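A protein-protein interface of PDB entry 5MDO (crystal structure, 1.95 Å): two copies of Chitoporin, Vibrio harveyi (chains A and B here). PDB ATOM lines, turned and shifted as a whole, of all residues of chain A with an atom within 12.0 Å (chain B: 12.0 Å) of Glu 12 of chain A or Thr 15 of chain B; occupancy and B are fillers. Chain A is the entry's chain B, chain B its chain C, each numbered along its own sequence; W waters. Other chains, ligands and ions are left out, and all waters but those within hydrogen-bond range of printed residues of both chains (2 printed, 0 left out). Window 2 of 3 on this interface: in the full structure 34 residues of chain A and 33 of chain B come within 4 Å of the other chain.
Of the 9 printed residues of chain A, 4 touch a printed residue of chain B. Printed residues of chain A that touch a printed residue of chain B: Glu 12, Tyr 13, Leu 14 and Tyr 21. Hydrophobic or aromatic side chains of chain A within 4 Å of the printed part of chain B: Tyr 13, Leu 14 and Tyr 21. Of the 12 printed residues of chain B, 6 touch a printed residue of chain A. Printed residues of chain B that touch a printed residue of chain A: Tyr 13, Leu 14, Thr 15, Lys 16, Phe 19 and Val 23. Among the printed residues, 9 pairs touch across the chains. Among the printed residues, no Asp or Glu carboxylate lies within 4 Å of a Lys or Arg side-chain nitrogen of the other chain.
Water W1 bridges OH of Tyr 21 of chain A and N of Val 23 of chain B. Water W2 bridges the side-chain hydroxyl (OH) of Tyr 21 of chain A and the side-chain hydroxyl (OH) of Tyr 21 of chain B.
Glu 12 of chain A touches Thr 15 of chain B, but with the chains exchanged Thr 15 of chain A does not touch Glu 12 of chain B (10.8 Å). Glu 12 of chain A touches Lys 16 of chain B, but with the chains exchanged Lys 16 of chain A does not touch Glu 12 of chain B (12.2 Å). Tyr 13 of chain A touches Leu 14 of chain B, but with the chains exchanged Leu 14 of chain A does not touch Tyr 13 of chain B (6.2 Å). Leu 14 of chain A touches Lys 16 of chain B, but with the chains exchanged Lys 16 of chain A does not touch Leu 14 of chain B (9.0 Å). Of the 9 pairs that touch across the chains among the printed residues, 2 have their exchanged pair printed and touching as well.
O of Leu 14 of chain B sits at hydrogen-bond distance from N of Leu 14 of chain A (3.1 Å).
Among the printed residues, pairs that only touch across the chains: Glu 12 of chain A with Thr 15 of chain B (3.2 Å), Glu 12 of chain A with Lys 16 of chain B (3.7 Å), Tyr 13 of chain A with Tyr 13 of chain B (3.7 Å), Tyr 13 of chain A with Leu 14 of chain B (3.5 Å), Leu 14 of chain A with Thr 15 of chain B (3.6 Å), Leu 14 of chain A with Lys 16 of chain B (3.95 Å), Leu 14 of chain A with Phe 19 of chain B (3.8 Å) and Tyr 21 of chain A with Val 23 of chain B (3.5 Å).
Of the printed residues of chain B, Glu 12 of chain A touches Thr 15 and Lys 16. Tyr 13 of chain A touches two residues of chain B. Thr 15 of chain A touches none of the printed residues of chain B. Phe 19 of chain A touches none of the printed residues of chain B. Of the printed residues of chain B, Tyr 21 of chain A touches Val 23. Of the printed residues of chain A, Tyr 13 of chain B touches Tyr 13 (3.7 Å). Of chain A, only Glu 12 (3.2 Å) and Leu 14 (3.6 Å) come within 4 Å of Thr 15 of chain B. No residue of chain A comes within 4 Å of Asp 17 of chain B. Of the printed residues of chain A, Val 23 of chain B touches Tyr 21 (3.5 Å).
The backbone NH of Thr 15 of chain B sits at hydrogen-bond distance from the side-chain hydroxyl of Ser 18 of chain B (2.8 Å). The backbone NH (N) of Asp 17 of chain B sits close to the side-chain hydroxyl (OG1) of Thr 15 of chain B, at 3.3 Å. The side-chain amino group (NZ) of Lys 16 of chain B is in salt-bridge range of the side-chain carboxylate (OE2) of Glu 22 of chain B, at 3.2 Å.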
ATOM      1  N   GLU A  12     -26.018   4.790  14.136  1.00  0.00           N
ATOM      2  CA  GLU A  12     -24.828   5.524  13.647  1.00  0.00           C
ATOM      3  C   GLU A  12     -24.013   6.188  14.796  1.00  0.00           C
ATOM      4  O   GLU A  12     -22.789   6.096  14.795  1.00  0.00           O
ATOM      5  CB  GLU A  12     -25.262   6.558  12.626  1.00  0.00           C
ATOM      6  CG  GLU A  12     -24.130   7.041  11.728  1.00  0.00           C
ATOM      7  CD  GLU A  12     -24.252   8.508  11.386  1.00  0.00           C
ATOM      8  OE1 GLU A  12     -23.337   9.040  10.729  1.00  0.00           O
ATOM      9  OE2 GLU A  12     -25.258   9.141  11.777  1.00  0.00           O
ATOM     10  N   TYR A  13     -24.694   6.839  15.751  1.00  0.00           N
ATOM     11  CA  TYR A  13     -24.056   7.473  16.926  1.00  0.00           C
ATOM     12  C   TYR A  13     -23.965   6.526  18.111  1.00  0.00           C
ATOM     13  O   TYR A  13     -24.916   5.818  18.422  1.00  0.00           O
ATOM     14  CB  TYR A  13     -24.796   8.732  17.372  1.00  0.00           C
ATOM     15  CG  TYR A  13     -24.614   9.877  16.412  1.00  0.00           C
ATOM     16  CD1 TYR A  13     -23.421  10.604  16.389  1.00  0.00           C
ATOM     17  CD2 TYR A  13     -25.633  10.240  15.502  1.00  0.00           C
ATOM     18  CE1 TYR A  13     -23.248  11.657  15.500  1.00  0.00           C
ATOM     19  CE2 TYR A  13     -25.464  11.298  14.614  1.00  0.00           C
ATOM     20  CZ  TYR A  13     -24.270  11.993  14.621  1.00  0.00           C
ATOM     21  OH  TYR A  13     -24.072  13.025  13.754  1.00  0.00           O
ATOM     22  N   LEU A  14     -22.825   6.528  18.790  1.00  0.00           N
ATOM     23  CA  LEU A  14     -22.567   5.570  19.867  1.00  0.00           C
ATOM     24  C   LEU A  14     -23.078   6.060  21.208  1.00  0.00           C
ATOM     25  O   LEU A  14     -23.090   7.256  21.486  1.00  0.00           O
ATOM     26  CB  LEU A  14     -21.062   5.293  19.986  1.00  0.00           C
ATOM     27  CG  LEU A  14     -20.334   4.859  18.719  1.00  0.00           C
ATOM     28  CD1 LEU A  14     -18.835   4.712  18.976  1.00  0.00           C
ATOM     29  CD2 LEU A  14     -20.939   3.575  18.162  1.00  0.00           C
ATOM     30  N   THR A  15     -23.484   5.096  22.053  1.00  0.00           N
ATOM     31  CA  THR A  15     -23.844   5.320  23.454  1.00  0.00           C
ATOM     32  C   THR A  15     -23.001   4.406  24.323  1.00  0.00           C
ATOM     33  O   THR A  15     -22.312   3.530  23.810  1.00  0.00           O
ATOM     34  CB  THR A  15     -25.359   5.037  23.738  1.00  0.00           C
ATOM     35  OG1 THR A  15     -25.661   3.649  23.544  1.00  0.00           O
ATOM     36  CG2 THR A  15     -26.269   5.854  22.804  1.00  0.00           C
ATOM     37  N   LYS A  16     -23.116   4.576  25.633  1.00  0.00           N
ATOM     38  CA  LYS A  16     -22.539   3.640  26.622  1.00  0.00           C
ATOM     39  C   LYS A  16     -22.862   2.157  26.300  1.00  0.00           C
ATOM     40  O   LYS A  16     -21.959   1.282  26.294  1.00  0.00           O
ATOM     41  CB  LYS A  16     -23.066   3.991  27.997  1.00  0.00           C
ATOM     42  CG  LYS A  16     -22.312   3.375  29.150  1.00  0.00           C
ATOM     43  CD  LYS A  16     -21.174   4.261  29.657  1.00  0.00           C
ATOM     44  CE  LYS A  16     -20.744   3.853  31.063  1.00  0.00           C
ATOM     45  NZ  LYS A  16     -19.518   3.003  31.042  1.00  0.00           N
ATOM     46  N   ASP A  17     -24.117   1.927  25.909  1.00  0.00           N
ATOM     47  CA  ASP A  17     -24.616   0.619  25.463  1.00  0.00           C
ATOM     48  C   ASP A  17     -24.050   0.070  24.207  1.00  0.00           C
ATOM     49  O   ASP A  17     -24.292  -1.074  23.917  1.00  0.00           O
ATOM     50  CB  ASP A  17     -26.155   0.683  25.207  1.00  0.00           C
ATOM     51  CG  ASP A  17     -26.941   1.038  26.445  1.00  0.00           C
ATOM     52  OD1 ASP A  17     -26.391   0.935  27.575  1.00  0.00           O
ATOM     53  OD2 ASP A  17     -28.124   1.418  26.284  1.00  0.00           O
ATOM     54  N   SER A  18     -23.384   0.857  23.387  1.00  0.00           N
ATOM     55  CA  SER A  18     -22.766   0.299  22.196  1.00  0.00           C
ATOM     56  C   SER A  18     -21.625  -0.665  22.506  1.00  0.00           C
ATOM     57  O   SER A  18     -21.200  -1.363  21.612  1.00  0.00           O
ATOM     58  CB  SER A  18     -22.197   1.410  21.308  1.00  0.00           C
ATOM     59  OG  SER A  18     -23.139   2.471  21.180  1.00  0.00           O
ATOM     60  N   PHE A  19     -21.044  -0.646  23.698  1.00  0.00           N
ATOM     61  CA  PHE A  19     -19.888  -1.499  23.987  1.00  0.00           C
ATOM     62  C   PHE A  19     -20.242  -2.514  25.032  1.00  0.00           C
ATOM     63  O   PHE A  19     -20.979  -2.177  25.937  1.00  0.00           O
ATOM     64  CB  PHE A  19     -18.698  -0.607  24.466  1.00  0.00           C
ATOM     65  CG  PHE A  19     -18.172   0.303  23.371  1.00  0.00           C
ATOM     66  CD1 PHE A  19     -17.452  -0.226  22.313  1.00  0.00           C
ATOM     67  CD2 PHE A  19     -18.515   1.645  23.333  1.00  0.00           C
ATOM     68  CE1 PHE A  19     -16.991   0.611  21.256  1.00  0.00           C
ATOM     69  CE2 PHE A  19     -18.071   2.486  22.314  1.00  0.00           C
ATOM     70  CZ  PHE A  19     -17.275   1.972  21.294  1.00  0.00           C
ATOM     71  N   TYR A  21     -17.821  -3.870  26.981  1.00  0.00           N
ATOM     72  CA  TYR A  21     -16.655  -3.899  27.791  1.00  0.00           C
ATOM     73  C   TYR A  21     -16.277  -2.441  28.109  1.00  0.00           C
ATOM     74  O   TYR A  21     -16.742  -1.530  27.446  1.00  0.00           O
ATOM     75  CB  TYR A  21     -15.426  -4.606  27.079  1.00  0.00           C
ATOM     76  CG  TYR A  21     -14.904  -3.770  25.963  1.00  0.00           C
ATOM     77  CD1 TYR A  21     -15.548  -3.743  24.749  1.00  0.00           C
ATOM     78  CD2 TYR A  21     -13.832  -2.838  26.188  1.00  0.00           C
ATOM     79  CE1 TYR A  21     -15.137  -2.901  23.712  1.00  0.00           C
ATOM     80  CE2 TYR A  21     -13.396  -1.999  25.173  1.00  0.00           C
ATOM     81  CZ  TYR A  21     -14.030  -2.009  23.942  1.00  0.00           C
ATOM     82  OH  TYR A  21     -13.659  -1.152  22.948  1.00  0.00           O
ATOM     83  N   GLU B  12     -17.563  16.123  17.154  1.00  0.00           N
ATOM     84  CA  GLU B  12     -17.704  16.016  18.632  1.00  0.00           C
ATOM     85  C   GLU B  12     -18.321  14.667  19.085  1.00  0.00           C
ATOM     86  O   GLU B  12     -17.818  14.057  20.040  1.00  0.00           O
ATOM     87  CB  GLU B  12     -18.534  17.182  19.144  1.00  0.00           C
ATOM     88  CG  GLU B  12     -18.366  17.451  20.634  1.00  0.00           C
ATOM     89  CD  GLU B  12     -19.649  17.905  21.292  1.00  0.00           C
ATOM     90  OE1 GLU B  12     -19.651  18.073  22.526  1.00  0.00           O
ATOM     91  OE2 GLU B  12     -20.659  18.076  20.580  1.00  0.00           O
ATOM     92  N   TYR B  13     -19.386  14.212  18.415  1.00  0.00           N
ATOM     93  CA  TYR B  13     -20.045  12.918  18.729  1.00  0.00           C
ATOM     94  C   TYR B  13     -19.455  11.755  17.948  1.00  0.00           C
ATOM     95  O   TYR B  13     -19.207  11.887  16.756  1.00  0.00           O
ATOM     96  CB  TYR B  13     -21.552  12.971  18.459  1.00  0.00           C
ATOM     97  CG  TYR B  13     -22.292  13.829  19.466  1.00  0.00           C
ATOM     98  CD1 TYR B  13     -22.534  13.357  20.763  1.00  0.00           C
ATOM     99  CD2 TYR B  13     -22.728  15.130  19.136  1.00  0.00           C
ATOM    100  CE1 TYR B  13     -23.211  14.142  21.692  1.00  0.00           C
ATOM    101  CE2 TYR B  13     -23.402  15.920  20.066  1.00  0.00           C
ATOM    102  CZ  TYR B  13     -23.633  15.416  21.333  1.00  0.00           C
ATOM    103  OH  TYR B  13     -24.278  16.169  22.258  1.00  0.00           O
ATOM    104  N   LEU B  14     -19.266  10.617  18.611  1.00  0.00           N
ATOM    105  CA  LEU B  14     -18.604   9.458  17.988  1.00  0.00           C
ATOM    106  C   LEU B  14     -19.563   8.576  17.208  1.00  0.00           C
ATOM    107  O   LEU B  14     -20.748   8.451  17.573  1.00  0.00           O
ATOM    108  CB  LEU B  14     -17.909   8.596  19.052  1.00  0.00           C
ATOM    109  CG  LEU B  14     -16.934   9.329  19.979  1.00  0.00           C
ATOM    110  CD1 LEU B  14     -16.390   8.371  21.029  1.00  0.00           C
ATOM    111  CD2 LEU B  14     -15.816   9.996  19.192  1.00  0.00           C
ATOM    112  N   THR B  15     -19.044   7.966  16.131  1.00  0.00           N
ATOM    113  CA  THR B  15     -19.755   6.955  15.343  1.00  0.00           C
ATOM    114  C   THR B  15     -18.893   5.726  15.264  1.00  0.00           C
ATOM    115  O   THR B  15     -17.751   5.748  15.701  1.00  0.00           O
ATOM    116  CB  THR B  15     -20.062   7.437  13.889  1.00  0.00           C
ATOM    117  OG1 THR B  15     -18.852   7.637  13.145  1.00  0.00           O
ATOM    118  CG2 THR B  15     -20.857   8.751  13.878  1.00  0.00           C
ATOM    119  N   LYS B  16     -19.431   4.662  14.675  1.00  0.00           N
ATOM    120  CA  LYS B  16     -18.680   3.449  14.358  1.00  0.00           C
ATOM    121  C   LYS B  16     -17.337   3.770  13.650  1.00  0.00           C
ATOM    122  O   LYS B  16     -16.271   3.234  14.027  1.00  0.00           O
ATOM    123  CB  LYS B  16     -19.533   2.541  13.479  1.00  0.00           C
ATOM    124  CG  LYS B  16     -19.034   1.114  13.352  1.00  0.00           C
ATOM    125  CD  LYS B  16     -19.627   0.189  14.404  1.00  0.00           C
ATOM    126  CE  LYS B  16     -19.492  -1.282  13.988  1.00  0.00           C
ATOM    127  NZ  LYS B  16     -18.340  -1.957  14.662  1.00  0.00           N
ATOM    128  N   ASP B  17     -17.412   4.693  12.698  1.00  0.00           N
ATOM    129  CA  ASP B  17     -16.272   5.206  11.935  1.00  0.00           C
ATOM    130  C   ASP B  17     -15.249   5.967  12.710  1.00  0.00           C
ATOM    131  O   ASP B  17     -14.208   6.231  12.167  1.00  0.00           O
ATOM    132  CB  ASP B  17     -16.748   6.189  10.836  1.00  0.00           C
ATOM    133  CG  ASP B  17     -17.634   5.530   9.806  1.00  0.00           C
ATOM    134  OD1 ASP B  17     -17.676   4.276   9.735  1.00  0.00           O
ATOM    135  OD2 ASP B  17     -18.304   6.271   9.057  1.00  0.00           O
ATOM    136  N   SER B  18     -15.541   6.419  13.926  1.00  0.00           N
ATOM    137  CA  SER B  18     -14.524   7.090  14.695  1.00  0.00           C
ATOM    138  C   SER B  18     -13.360   6.165  15.088  1.00  0.00           C
ATOM    139  O   SER B  18     -12.357   6.684  15.519  1.00  0.00           O
ATOM    140  CB  SER B  18     -15.115   7.685  15.981  1.00  0.00           C
ATOM    141  OG  SER B  18     -16.337   8.338  15.706  1.00  0.00           O
ATOM    142  N   PHE B  19     -13.524   4.840  15.084  1.00  0.00           N
ATOM    143  CA  PHE B  19     -12.489   3.942  15.576  1.00  0.00           C
ATOM    144  C   PHE B  19     -11.986   3.107  14.414  1.00  0.00           C
ATOM    145  O   PHE B  19     -12.749   2.738  13.568  1.00  0.00           O
ATOM    146  CB  PHE B  19     -13.025   3.051  16.688  1.00  0.00           C
ATOM    147  CG  PHE B  19     -13.391   3.804  17.935  1.00  0.00           C
ATOM    148  CD1 PHE B  19     -12.374   4.375  18.732  1.00  0.00           C
ATOM    149  CD2 PHE B  19     -14.722   4.133  18.212  1.00  0.00           C
ATOM    150  CE1 PHE B  19     -12.690   5.147  19.868  1.00  0.00           C
ATOM    151  CE2 PHE B  19     -15.053   4.855  19.357  1.00  0.00           C
ATOM    152  CZ  PHE B  19     -14.029   5.347  20.191  1.00  0.00           C
ATOM    153  N   SER B  20     -10.706   2.818  14.401  1.00  0.00           N
ATOM    154  CA  SER B  20     -10.099   1.933  13.382  1.00  0.00           C
ATOM    155  C   SER B  20      -9.895   0.507  13.839  1.00  0.00           C
ATOM    156  O   SER B  20      -9.144  -0.245  13.231  1.00  0.00           O
ATOM    157  CB  SER B  20      -8.736   2.556  12.971  1.00  0.00           C
ATOM    158  OG  SER B  20      -9.032   3.834  12.440  1.00  0.00           O
ATOM    159  N   TYR B  21     -10.463   0.143  15.008  1.00  0.00           N
ATOM    160  CA  TYR B  21     -10.287  -1.134  15.579  1.00  0.00           C
ATOM    161  C   TYR B  21     -11.635  -1.468  16.362  1.00  0.00           C
ATOM    162  O   TYR B  21     -12.421  -0.586  16.630  1.00  0.00           O
ATOM    163  CB  TYR B  21      -9.106  -1.189  16.554  1.00  0.00           C
ATOM    164  CG  TYR B  21      -9.403  -0.396  17.796  1.00  0.00           C
ATOM    165  CD1 TYR B  21      -9.268   0.986  17.808  1.00  0.00           C
ATOM    166  CD2 TYR B  21      -9.928  -1.016  18.951  1.00  0.00           C
ATOM    167  CE1 TYR B  21      -9.643   1.760  18.912  1.00  0.00           C
ATOM    168  CE2 TYR B  21     -10.275  -0.246  20.073  1.00  0.00           C
ATOM    169  CZ  TYR B  21     -10.140   1.131  20.061  1.00  0.00           C
ATOM    170  OH  TYR B  21     -10.496   1.879  21.143  1.00  0.00           O
ATOM    171  N   GLU B  22     -11.815  -2.736  16.611  1.00  0.00           N
ATOM    172  CA  GLU B  22     -12.834  -3.248  17.530  1.00  0.00           C
ATOM    173  C   GLU B  22     -12.134  -4.190  18.492  1.00  0.00           C
ATOM    174  O   GLU B  22     -11.390  -5.040  18.121  1.00  0.00           O
ATOM    175  CB  GLU B  22     -13.879  -4.209  16.921  1.00  0.00           C
ATOM    176  CG  GLU B  22     -14.616  -3.822  15.771  1.00  0.00           C
ATOM    177  CD  GLU B  22     -15.629  -4.939  15.454  1.00  0.00           C
ATOM    178  OE1 GLU B  22     -15.278  -6.134  15.190  1.00  0.00           O
ATOM    179  OE2 GLU B  22     -16.786  -4.551  15.624  1.00  0.00           O
ATOM    180  N   VAL B  23     -12.564  -4.097  19.732  1.00  0.00           N
ATOM    181  CA  VAL B  23     -12.222  -5.084  20.796  1.00  0.00           C
ATOM    182  C   VAL B  23     -13.311  -6.139  20.735  1.00  0.00           C
ATOM    183  O   VAL B  23     -14.460  -5.826  20.573  1.00  0.00           O
ATOM    184  CB  VAL B  23     -12.145  -4.436  22.168  1.00  0.00           C
ATOM    185  CG1 VAL B  23     -12.005  -5.502  23.276  1.00  0.00           C
ATOM    186  CG2 VAL B  23     -10.948  -3.502  22.207  1.00  0.00           C
HETATM  187  O   HOH W   1     -14.353  -1.917  20.480  1.00  0.00           O
HETATM  188  O   HOH W   2     -11.523   0.518  23.385  1.00  0.00           O
